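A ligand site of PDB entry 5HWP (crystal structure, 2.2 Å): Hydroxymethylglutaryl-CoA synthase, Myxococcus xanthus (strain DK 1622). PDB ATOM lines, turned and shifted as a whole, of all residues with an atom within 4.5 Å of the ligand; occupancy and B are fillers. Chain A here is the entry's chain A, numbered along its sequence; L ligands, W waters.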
ATOM      1  N   ASP A  33     -15.462 -11.886  16.461  1.00  0.00           N
ATOM      2  CA  ASP A  33     -15.205 -10.476  16.205  1.00  0.00           C
ATOM      3  C   ASP A  33     -15.624 -10.134  14.774  1.00  0.00           C
ATOM      4  O   ASP A  33     -15.084 -10.731  13.830  1.00  0.00           O
ATOM      5  CB  ASP A  33     -13.722 -10.169  16.414  1.00  0.00           C
ATOM      6  CG  ASP A  33     -13.408  -8.690  16.335  1.00  0.00           C
ATOM      7  OD1 ASP A  33     -14.114  -7.959  15.612  1.00  0.00           O
ATOM      8  OD2 ASP A  33     -12.451  -8.246  17.005  1.00  0.00           O
ATOM      9  N   ALA A  35     -14.764  -7.939  12.754  1.00  0.00           N
ATOM     10  CA  ALA A  35     -13.652  -7.567  11.889  1.00  0.00           C
ATOM     11  C   ALA A  35     -12.983  -8.775  11.261  1.00  0.00           C
ATOM     12  O   ALA A  35     -12.297  -8.625  10.233  1.00  0.00           O
ATOM     13  CB  ALA A  35     -12.627  -6.750  12.682  1.00  0.00           C
ATOM     14  N   LYS A  36     -13.131  -9.965  11.839  1.00  0.00           N
ATOM     15  CA  LYS A  36     -12.551 -11.151  11.233  1.00  0.00           C
ATOM     16  C   LYS A  36     -13.173 -11.432   9.870  1.00  0.00           C
ATOM     17  O   LYS A  36     -12.477 -11.780   8.913  1.00  0.00           O
ATOM     18  CB  LYS A  36     -12.701 -12.372  12.143  1.00  0.00           C
ATOM     19  CG  LYS A  36     -12.189 -13.655  11.512  1.00  0.00           C
ATOM     20  CD  LYS A  36     -12.214 -14.840  12.465  1.00  0.00           C
ATOM     21  CE  LYS A  36     -11.659 -16.087  11.774  1.00  0.00           C
ATOM     22  NZ  LYS A  36     -11.667 -17.287  12.647  1.00  0.00           N
ATOM     23  N   ALA A  39     -12.709  -7.578   7.650  1.00  0.00           N
ATOM     24  CA  ALA A  39     -11.318  -7.302   7.311  1.00  0.00           C
ATOM     25  C   ALA A  39     -10.541  -8.580   7.021  1.00  0.00           C
ATOM     26  O   ALA A  39      -9.812  -8.659   6.033  1.00  0.00           O
ATOM     27  CB  ALA A  39     -10.641  -6.529   8.454  1.00  0.00           C
ATOM     28  N   GLY A  40     -10.695  -9.595   7.879  1.00  0.00           N
ATOM     29  CA  GLY A  40      -9.934 -10.819   7.710  1.00  0.00           C
ATOM     30  C   GLY A  40     -10.289 -11.570   6.444  1.00  0.00           C
ATOM     31  O   GLY A  40      -9.416 -12.092   5.750  1.00  0.00           O
ATOM     32  N   LEU A  41     -11.588 -11.635   6.127  1.00  0.00           N
ATOM     33  CA  LEU A  41     -12.058 -12.358   4.955  1.00  0.00           C
ATOM     34  C   LEU A  41     -12.503 -11.456   3.814  1.00  0.00           C
ATOM     35  O   LEU A  41     -12.540 -11.911   2.662  1.00  0.00           O
ATOM     36  CB  LEU A  41     -13.219 -13.289   5.324  1.00  0.00           C
ATOM     37  CG  LEU A  41     -12.925 -14.331   6.404  1.00  0.00           C
ATOM     38  CD1 LEU A  41     -14.160 -15.183   6.658  1.00  0.00           C
ATOM     39  CD2 LEU A  41     -11.733 -15.212   6.019  1.00  0.00           C
ATOM     40  N   SCY A 117     -14.799 -26.172  -7.684  1.00  0.00           N
ATOM     41  CA  SCY A 117     -15.022 -24.825  -8.189  1.00  0.00           C
ATOM     42  CB  SCY A 117     -14.524 -23.796  -7.170  1.00  0.00           C
ATOM     43  SG  SCY A 117     -13.314 -24.515  -6.025  1.00  0.00           S
ATOM     44  CD  SCY A 117     -13.918 -24.404  -4.314  1.00  0.00           C
ATOM     45  OCD SCY A 117     -13.769 -23.405  -3.690  1.00  0.00           O
ATOM     46  CE  SCY A 117     -14.607 -25.612  -3.691  1.00  0.00           C
ATOM     47  C   SCY A 117     -14.333 -24.580  -9.549  1.00  0.00           C
ATOM     48  O   SCY A 117     -14.315 -23.420 -10.027  1.00  0.00           O
ATOM     49  N   TYR A 151     -21.432 -25.052   4.251  1.00  0.00           N
ATOM     50  CA  TYR A 151     -20.504 -25.669   5.181  1.00  0.00           C
ATOM     51  C   TYR A 151     -21.141 -26.085   6.501  1.00  0.00           C
ATOM     52  O   TYR A 151     -20.662 -27.021   7.133  1.00  0.00           O
ATOM     53  CB  TYR A 151     -19.332 -24.713   5.472  1.00  0.00           C
ATOM     54  CG  TYR A 151     -18.438 -24.492   4.281  1.00  0.00           C
ATOM     55  CD1 TYR A 151     -17.408 -25.374   3.992  1.00  0.00           C
ATOM     56  CD2 TYR A 151     -18.607 -23.402   3.441  1.00  0.00           C
ATOM     57  CE1 TYR A 151     -16.576 -25.183   2.900  1.00  0.00           C
ATOM     58  CE2 TYR A 151     -17.787 -23.192   2.350  1.00  0.00           C
ATOM     59  CZ  TYR A 151     -16.768 -24.093   2.083  1.00  0.00           C
ATOM     60  OH  TYR A 151     -15.952 -23.886   1.001  1.00  0.00           O
ATOM     61  N   ALA A 156     -15.999 -23.433  10.423  1.00  0.00           N
ATOM     62  CA  ALA A 156     -15.058 -22.401  10.003  1.00  0.00           C
ATOM     63  C   ALA A 156     -15.404 -21.871   8.612  1.00  0.00           C
ATOM     64  O   ALA A 156     -15.132 -20.701   8.318  1.00  0.00           O
ATOM     65  CB  ALA A 156     -13.635 -22.951  10.012  1.00  0.00           C
ATOM     66  N   GLY A 157     -15.982 -22.710   7.757  1.00  0.00           N
ATOM     67  CA  GLY A 157     -16.333 -22.292   6.415  1.00  0.00           C
ATOM     68  C   GLY A 157     -17.647 -21.552   6.287  1.00  0.00           C
ATOM     69  O   GLY A 157     -17.921 -20.997   5.217  1.00  0.00           O
ATOM     70  N   THR A 160     -17.931 -18.103   4.570  1.00  0.00           N
ATOM     71  CA  THR A 160     -17.616 -18.081   3.143  1.00  0.00           C
ATOM     72  C   THR A 160     -18.716 -18.736   2.305  1.00  0.00           C
ATOM     73  O   THR A 160     -18.505 -18.974   1.116  1.00  0.00           O
ATOM     74  CB  THR A 160     -16.275 -18.764   2.868  1.00  0.00           C
ATOM     75  OG1 THR A 160     -16.415 -20.180   3.026  1.00  0.00           O
ATOM     76  CG2 THR A 160     -15.196 -18.250   3.808  1.00  0.00           C
ATOM     77  N   VAL A 205     -13.677 -29.907   4.685  1.00  0.00           N
ATOM     78  CA  VAL A 205     -12.602 -29.028   4.239  1.00  0.00           C
ATOM     79  C   VAL A 205     -11.519 -28.978   5.309  1.00  0.00           C
ATOM     80  O   VAL A 205     -11.794 -28.901   6.509  1.00  0.00           O
ATOM     81  CB  VAL A 205     -13.147 -27.610   3.928  1.00  0.00           C
ATOM     82  CG1 VAL A 205     -13.690 -26.934   5.189  1.00  0.00           C
ATOM     83  CG2 VAL A 205     -12.069 -26.771   3.278  1.00  0.00           C
ATOM     84  N   GLY A 207      -9.287 -26.296   5.981  1.00  0.00           N
ATOM     85  CA  GLY A 207      -9.257 -24.903   5.576  1.00  0.00           C
ATOM     86  C   GLY A 207      -7.934 -24.373   5.074  1.00  0.00           C
ATOM     87  O   GLY A 207      -7.800 -24.013   3.902  1.00  0.00           O
ATOM     88  N   HIS A 208      -6.935 -24.297   5.956  1.00  0.00           N
ATOM     89  CA  HIS A 208      -5.655 -23.718   5.583  1.00  0.00           C
ATOM     90  C   HIS A 208      -4.891 -24.601   4.607  1.00  0.00           C
ATOM     91  O   HIS A 208      -4.036 -24.097   3.876  1.00  0.00           O
ATOM     92  CB  HIS A 208      -4.816 -23.443   6.830  1.00  0.00           C
ATOM     93  CG  HIS A 208      -5.345 -22.322   7.663  1.00  0.00           C
ATOM     94  ND1 HIS A 208      -6.274 -22.508   8.659  1.00  0.00           N
ATOM     95  CD2 HIS A 208      -5.089 -20.992   7.626  1.00  0.00           C
ATOM     96  CE1 HIS A 208      -6.561 -21.340   9.219  1.00  0.00           C
ATOM     97  NE2 HIS A 208      -5.858 -20.407   8.602  1.00  0.00           N
ATOM     98  N   SER A 210      -6.437 -26.168   2.105  1.00  0.00           N
ATOM     99  CA  SER A 210      -7.003 -25.806   0.808  1.00  0.00           C
ATOM    100  C   SER A 210      -6.405 -24.514   0.277  1.00  0.00           C
ATOM    101  O   SER A 210      -6.293 -24.342  -0.945  1.00  0.00           O
ATOM    102  CB  SER A 210      -8.527 -25.679   0.915  1.00  0.00           C
ATOM    103  OG  SER A 210      -8.904 -24.519   1.628  1.00  0.00           O
ATOM    104  N   ILE A 211      -6.018 -23.604   1.157  1.00  0.00           N
ATOM    105  CA  ILE A 211      -5.341 -22.387   0.733  1.00  0.00           C
ATOM    106  C   ILE A 211      -3.989 -22.728   0.120  1.00  0.00           C
ATOM    107  O   ILE A 211      -3.618 -22.210  -0.940  1.00  0.00           O
ATOM    108  CB  ILE A 211      -5.199 -21.408   1.918  1.00  0.00           C
ATOM    109  CG1 ILE A 211      -6.578 -20.837   2.263  1.00  0.00           C
ATOM    110  CG2 ILE A 211      -4.217 -20.275   1.597  1.00  0.00           C
ATOM    111  CD1 ILE A 211      -6.619 -20.075   3.578  1.00  0.00           C
ATOM    112  N   TYR A 214      -4.503 -24.316  -3.215  1.00  0.00           N
ATOM    113  CA  TYR A 214      -4.842 -23.245  -4.140  1.00  0.00           C
ATOM    114  C   TYR A 214      -3.587 -22.575  -4.681  1.00  0.00           C
ATOM    115  O   TYR A 214      -3.390 -22.467  -5.897  1.00  0.00           O
ATOM    116  CB  TYR A 214      -5.754 -22.233  -3.440  1.00  0.00           C
ATOM    117  CG  TYR A 214      -6.269 -21.086  -4.283  1.00  0.00           C
ATOM    118  CD1 TYR A 214      -5.409 -20.128  -4.809  1.00  0.00           C
ATOM    119  CD2 TYR A 214      -7.627 -20.931  -4.521  1.00  0.00           C
ATOM    120  CE1 TYR A 214      -5.877 -19.075  -5.569  1.00  0.00           C
ATOM    121  CE2 TYR A 214      -8.108 -19.881  -5.277  1.00  0.00           C
ATOM    122  CZ  TYR A 214      -7.231 -18.955  -5.795  1.00  0.00           C
ATOM    123  OH  TYR A 214      -7.704 -17.905  -6.546  1.00  0.00           O
ATOM    124  N   PRO A 254     -12.868 -17.832  -3.255  1.00  0.00           N
ATOM    125  CA  PRO A 254     -13.606 -18.486  -2.165  1.00  0.00           C
ATOM    126  C   PRO A 254     -13.977 -17.498  -1.075  1.00  0.00           C
ATOM    127  O   PRO A 254     -15.028 -17.625  -0.452  1.00  0.00           O
ATOM    128  CB  PRO A 254     -12.635 -19.554  -1.663  1.00  0.00           C
ATOM    129  CG  PRO A 254     -11.281 -19.002  -1.985  1.00  0.00           C
ATOM    130  CD  PRO A 254     -11.443 -18.226  -3.267  1.00  0.00           C
ATOM    131  N   PHE A 255     -13.105 -16.517  -0.834  1.00  0.00           N
ATOM    132  CA  PHE A 255     -13.406 -15.344  -0.028  1.00  0.00           C
ATOM    133  C   PHE A 255     -12.542 -14.208  -0.578  1.00  0.00           C
ATOM    134  O   PHE A 255     -11.514 -14.451  -1.214  1.00  0.00           O
ATOM    135  CB  PHE A 255     -13.152 -15.580   1.466  1.00  0.00           C
ATOM    136  CG  PHE A 255     -11.781 -16.116   1.775  1.00  0.00           C
ATOM    137  CD1 PHE A 255     -11.492 -17.460   1.601  1.00  0.00           C
ATOM    138  CD2 PHE A 255     -10.789 -15.273   2.238  1.00  0.00           C
ATOM    139  CE1 PHE A 255     -10.230 -17.950   1.884  1.00  0.00           C
ATOM    140  CE2 PHE A 255      -9.529 -15.754   2.524  1.00  0.00           C
ATOM    141  CZ  PHE A 255      -9.249 -17.097   2.346  1.00  0.00           C
ATOM    142  N   LYS A 261      -3.901 -12.890  -1.569  1.00  0.00           N
ATOM    143  CA  LYS A 261      -2.967 -14.005  -1.438  1.00  0.00           C
ATOM    144  C   LYS A 261      -2.570 -14.541  -2.803  1.00  0.00           C
ATOM    145  O   LYS A 261      -1.386 -14.757  -3.084  1.00  0.00           O
ATOM    146  CB  LYS A 261      -3.590 -15.117  -0.587  1.00  0.00           C
ATOM    147  CG  LYS A 261      -4.049 -14.687   0.787  1.00  0.00           C
ATOM    148  CD  LYS A 261      -4.556 -15.881   1.582  1.00  0.00           C
ATOM    149  CE  LYS A 261      -5.013 -15.468   2.974  1.00  0.00           C
ATOM    150  NZ  LYS A 261      -3.973 -14.678   3.692  1.00  0.00           N
ATOM    151  N   TYR A 342      -9.555 -22.184 -10.020  1.00  0.00           N
ATOM    152  CA  TYR A 342      -9.139 -23.252  -9.138  1.00  0.00           C
ATOM    153  C   TYR A 342     -10.308 -24.144  -8.794  1.00  0.00           C
ATOM    154  O   TYR A 342     -11.457 -23.685  -8.661  1.00  0.00           O
ATOM    155  CB  TYR A 342      -8.512 -22.716  -7.839  1.00  0.00           C
ATOM    156  CG  TYR A 342      -8.107 -23.816  -6.892  1.00  0.00           C
ATOM    157  CD1 TYR A 342      -6.975 -24.586  -7.156  1.00  0.00           C
ATOM    158  CD2 TYR A 342      -8.834 -24.095  -5.744  1.00  0.00           C
ATOM    159  CE1 TYR A 342      -6.592 -25.599  -6.293  1.00  0.00           C
ATOM    160  CE2 TYR A 342      -8.460 -25.108  -4.886  1.00  0.00           C
ATOM    161  CZ  TYR A 342      -7.331 -25.852  -5.165  1.00  0.00           C
ATOM    162  OH  TYR A 342      -6.957 -26.865  -4.307  1.00  0.00           O
ATOM    163  N   SER A 344     -10.900 -27.364  -5.927  1.00  0.00           N
ATOM    164  CA  SER A 344     -10.394 -28.286  -4.929  1.00  0.00           C
ATOM    165  C   SER A 344     -10.488 -29.711  -5.454  1.00  0.00           C
ATOM    166  O   SER A 344     -11.429 -30.062  -6.175  1.00  0.00           O
ATOM    167  CB  SER A 344     -11.173 -28.147  -3.620  1.00  0.00           C
ATOM    168  OG  SER A 344     -11.030 -26.852  -3.062  1.00  0.00           O
HETATM  169  N1  LIG L   1      -9.412  -8.362  12.882  1.00  0.00           N
HETATM  170  C1  LIG L   1      -8.791  -8.475  11.752  1.00  0.00           C
HETATM  171  N2  LIG L   1      -8.438  -9.625  11.197  1.00  0.00           N
HETATM  172  C2  LIG L   1      -8.713 -10.757  11.803  1.00  0.00           C
HETATM  173  C3  LIG L   1      -9.397 -10.734  13.055  1.00  0.00           C
HETATM  174  C4  LIG L   1      -9.750  -9.410  13.595  1.00  0.00           C
HETATM  175  N3  LIG L   1     -10.369  -9.282  14.744  1.00  0.00           N
HETATM  176  N4  LIG L   1      -9.531 -11.977  13.405  1.00  0.00           N
HETATM  177  C5  LIG L   1      -9.015 -12.755  12.521  1.00  0.00           C
HETATM  178  N5  LIG L   1      -8.520 -12.038  11.556  1.00  0.00           N
HETATM  179  C6  LIG L   1      -7.824 -12.457  10.356  1.00  0.00           C
HETATM  180  C7  LIG L   1      -6.709 -13.482  10.556  1.00  0.00           C
HETATM  181  O1  LIG L   1      -5.521 -12.998  11.040  1.00  0.00           O
HETATM  182  C8  LIG L   1      -6.548 -14.115   9.187  1.00  0.00           C
HETATM  183  O2  LIG L   1      -5.689 -13.350   8.369  1.00  0.00           O
HETATM  184  P1  LIG L   1      -4.754 -13.676   7.187  1.00  0.00           P
HETATM  185  O3  LIG L   1      -3.721 -14.396   7.822  1.00  0.00           O
HETATM  186  O4  LIG L   1      -5.465 -14.411   6.244  1.00  0.00           O
HETATM  187  O5  LIG L   1      -4.402 -12.450   6.587  1.00  0.00           O
HETATM  188  C9  LIG L   1      -7.959 -14.071   8.675  1.00  0.00           C
HETATM  189  O6  LIG L   1      -8.666 -13.045   9.391  1.00  0.00           O
HETATM  190  C10 LIG L   1      -8.614 -15.443   8.763  1.00  0.00           C
HETATM  191  O7  LIG L   1      -8.494 -16.101  10.022  1.00  0.00           O
HETATM  192  P2  LIG L   1      -8.290 -17.662  10.160  1.00  0.00           P
HETATM  193  O8  LIG L   1      -7.937 -18.148  11.452  1.00  0.00           O
HETATM  194  O9  LIG L   1      -7.446 -18.044   9.111  1.00  0.00           O
HETATM  195  O10 LIG L   1      -9.769 -18.085   9.919  1.00  0.00           O
HETATM  196  P3  LIG L   1     -10.404 -19.494   9.967  1.00  0.00           P
HETATM  197  O11 LIG L   1      -9.443 -20.551   9.896  1.00  0.00           O
HETATM  198  O12 LIG L   1     -11.476 -19.629  10.873  1.00  0.00           O
HETATM  199  O13 LIG L   1     -11.145 -19.636   8.644  1.00  0.00           O
HETATM  200  C11 LIG L   1     -10.953 -20.196   6.293  1.00  0.00           C
HETATM  201  C12 LIG L   1     -10.576 -19.276   7.434  1.00  0.00           C
HETATM  202  C13 LIG L   1     -10.999 -19.441   5.027  1.00  0.00           C
HETATM  203  C14 LIG L   1      -9.893 -21.233   6.138  1.00  0.00           C
HETATM  204  C15 LIG L   1     -12.314 -20.876   6.514  1.00  0.00           C
HETATM  205  O14 LIG L   1     -13.287 -19.916   6.386  1.00  0.00           O
HETATM  206  C16 LIG L   1     -12.574 -22.000   5.533  1.00  0.00           C
HETATM  207  O15 LIG L   1     -12.166 -23.073   5.729  1.00  0.00           O
HETATM  208  N6  LIG L   1     -13.281 -21.752   4.464  1.00  0.00           N
HETATM  209  C17 LIG L   1     -13.737 -22.729   3.498  1.00  0.00           C
HETATM  210  C18 LIG L   1     -12.792 -23.186   2.401  1.00  0.00           C
HETATM  211  C19 LIG L   1     -12.164 -22.075   1.588  1.00  0.00           C
HETATM  212  O16 LIG L   1     -12.760 -21.121   1.248  1.00  0.00           O
HETATM  213  N7  LIG L   1     -10.906 -22.215   1.231  1.00  0.00           N
HETATM  214  C20 LIG L   1     -10.207 -21.300   0.402  1.00  0.00           C
HETATM  215  C21 LIG L   1      -9.328 -21.958  -0.593  1.00  0.00           C
HETATM  216  S1  LIG L   1     -10.331 -22.649  -1.909  1.00  0.00           S
HETATM  217  O   HOH W   1      -2.942 -11.965   9.658  1.00  0.00           O
HETATM  218  O   HOH W   2      -6.961  -8.913   8.795  1.00  0.00           O
HETATM  219  O   HOH W   3      -9.995 -23.171   9.893  1.00  0.00           O
HETATM  220  O   HOH W   4     -14.351 -18.722  10.179  1.00  0.00           O
HETATM  221  O   HOH W   5      -7.765 -14.362   5.011  1.00  0.00           O
HETATM  222  O   HOH W   6      -4.736 -17.649  10.899  1.00  0.00           O
HETATM  223  O   HOH W   7     -11.424 -24.593   7.783  1.00  0.00           O
HETATM  224  O   HOH W   8     -15.378 -21.374   0.889  1.00  0.00           O
HETATM  225  O   HOH W   9     -10.812 -12.332  15.941  1.00  0.00           O
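An oxygen (O9) of the ligand is in hydrogen-bond range of a ring nitrogen (NE2) of His 208 (2.9 Å).
The side-chain amino group (NZ) of Lys 261 lies within salt-bridge range of an oxygen (O4) of the ligand.
N7 of the ligand lies within hydrogen-bond range of OG of Ser 210 (3.1 Å).
O14 of the ligand lies within hydrogen-bond range of O of Ala 156.
OD2 of Asp 33 is in hydrogen-bond range of N3 of the ligand (3.2 Å).
NZ of Lys 36 lies within salt-bridge range of O12 of the ligand (2.9 Å).
The side-chain carboxylate of Asp 33 sits at hydrogen-bond distance from the backbone NH of Ala 35, at 2.9 Å.
The backbone carbonyl oxygen (O) of Ala 35 lies within hydrogen-bond range of the backbone NH (N) of Gly 40 (3.0 Å).
SG of SCY 117 sits at hydrogen-bond distance from the backbone NH (N) of Ser 344, at 3.7 Å.
The side-chain hydroxyl (OG) of Ser 210 lies within hydrogen-bond range of the backbone carbonyl oxygen (O) of Gly 207.
OG1 of Thr 160 lies within hydrogen-bond range of O of Gly 157, 2.8 Å away.
N of Leu 41 is in hydrogen-bond range of O of Lys 36, at 2.9 Å.
Residues that only touch the ligand: Ala 35, Gly 40, SCY 117, Tyr 151, Gly 157, Thr 160, Val 205, Gly 207, Pro 254 and Phe 255.
Hydrophobic or aromatic side chains that line the ligand: Ala 35, Tyr 151, Val 205, His 208, Pro 254 and Phe 255.
Along chain A the residues within 4 Å of the ligand span positions 33 to 261.
Water W5 lies within hydrogen-bond range of an oxygen (O4) of the ligand (2.6 Å) and the backbone carbonyl oxygen (O) of Gly 40 (2.9 Å).
Water W8 lies within hydrogen-bond range of OH of Tyr 151, O16 of the ligand and OG1 of Thr 160.
Water W7 lies within hydrogen-bond range of an oxygen (O15) of the ligand (2.7 Å) and the backbone NH of Gly 207 (3.3 Å).
Water W4 bridges the backbone carbonyl oxygen of Ala 156 and an oxygen (O12) of the ligand.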
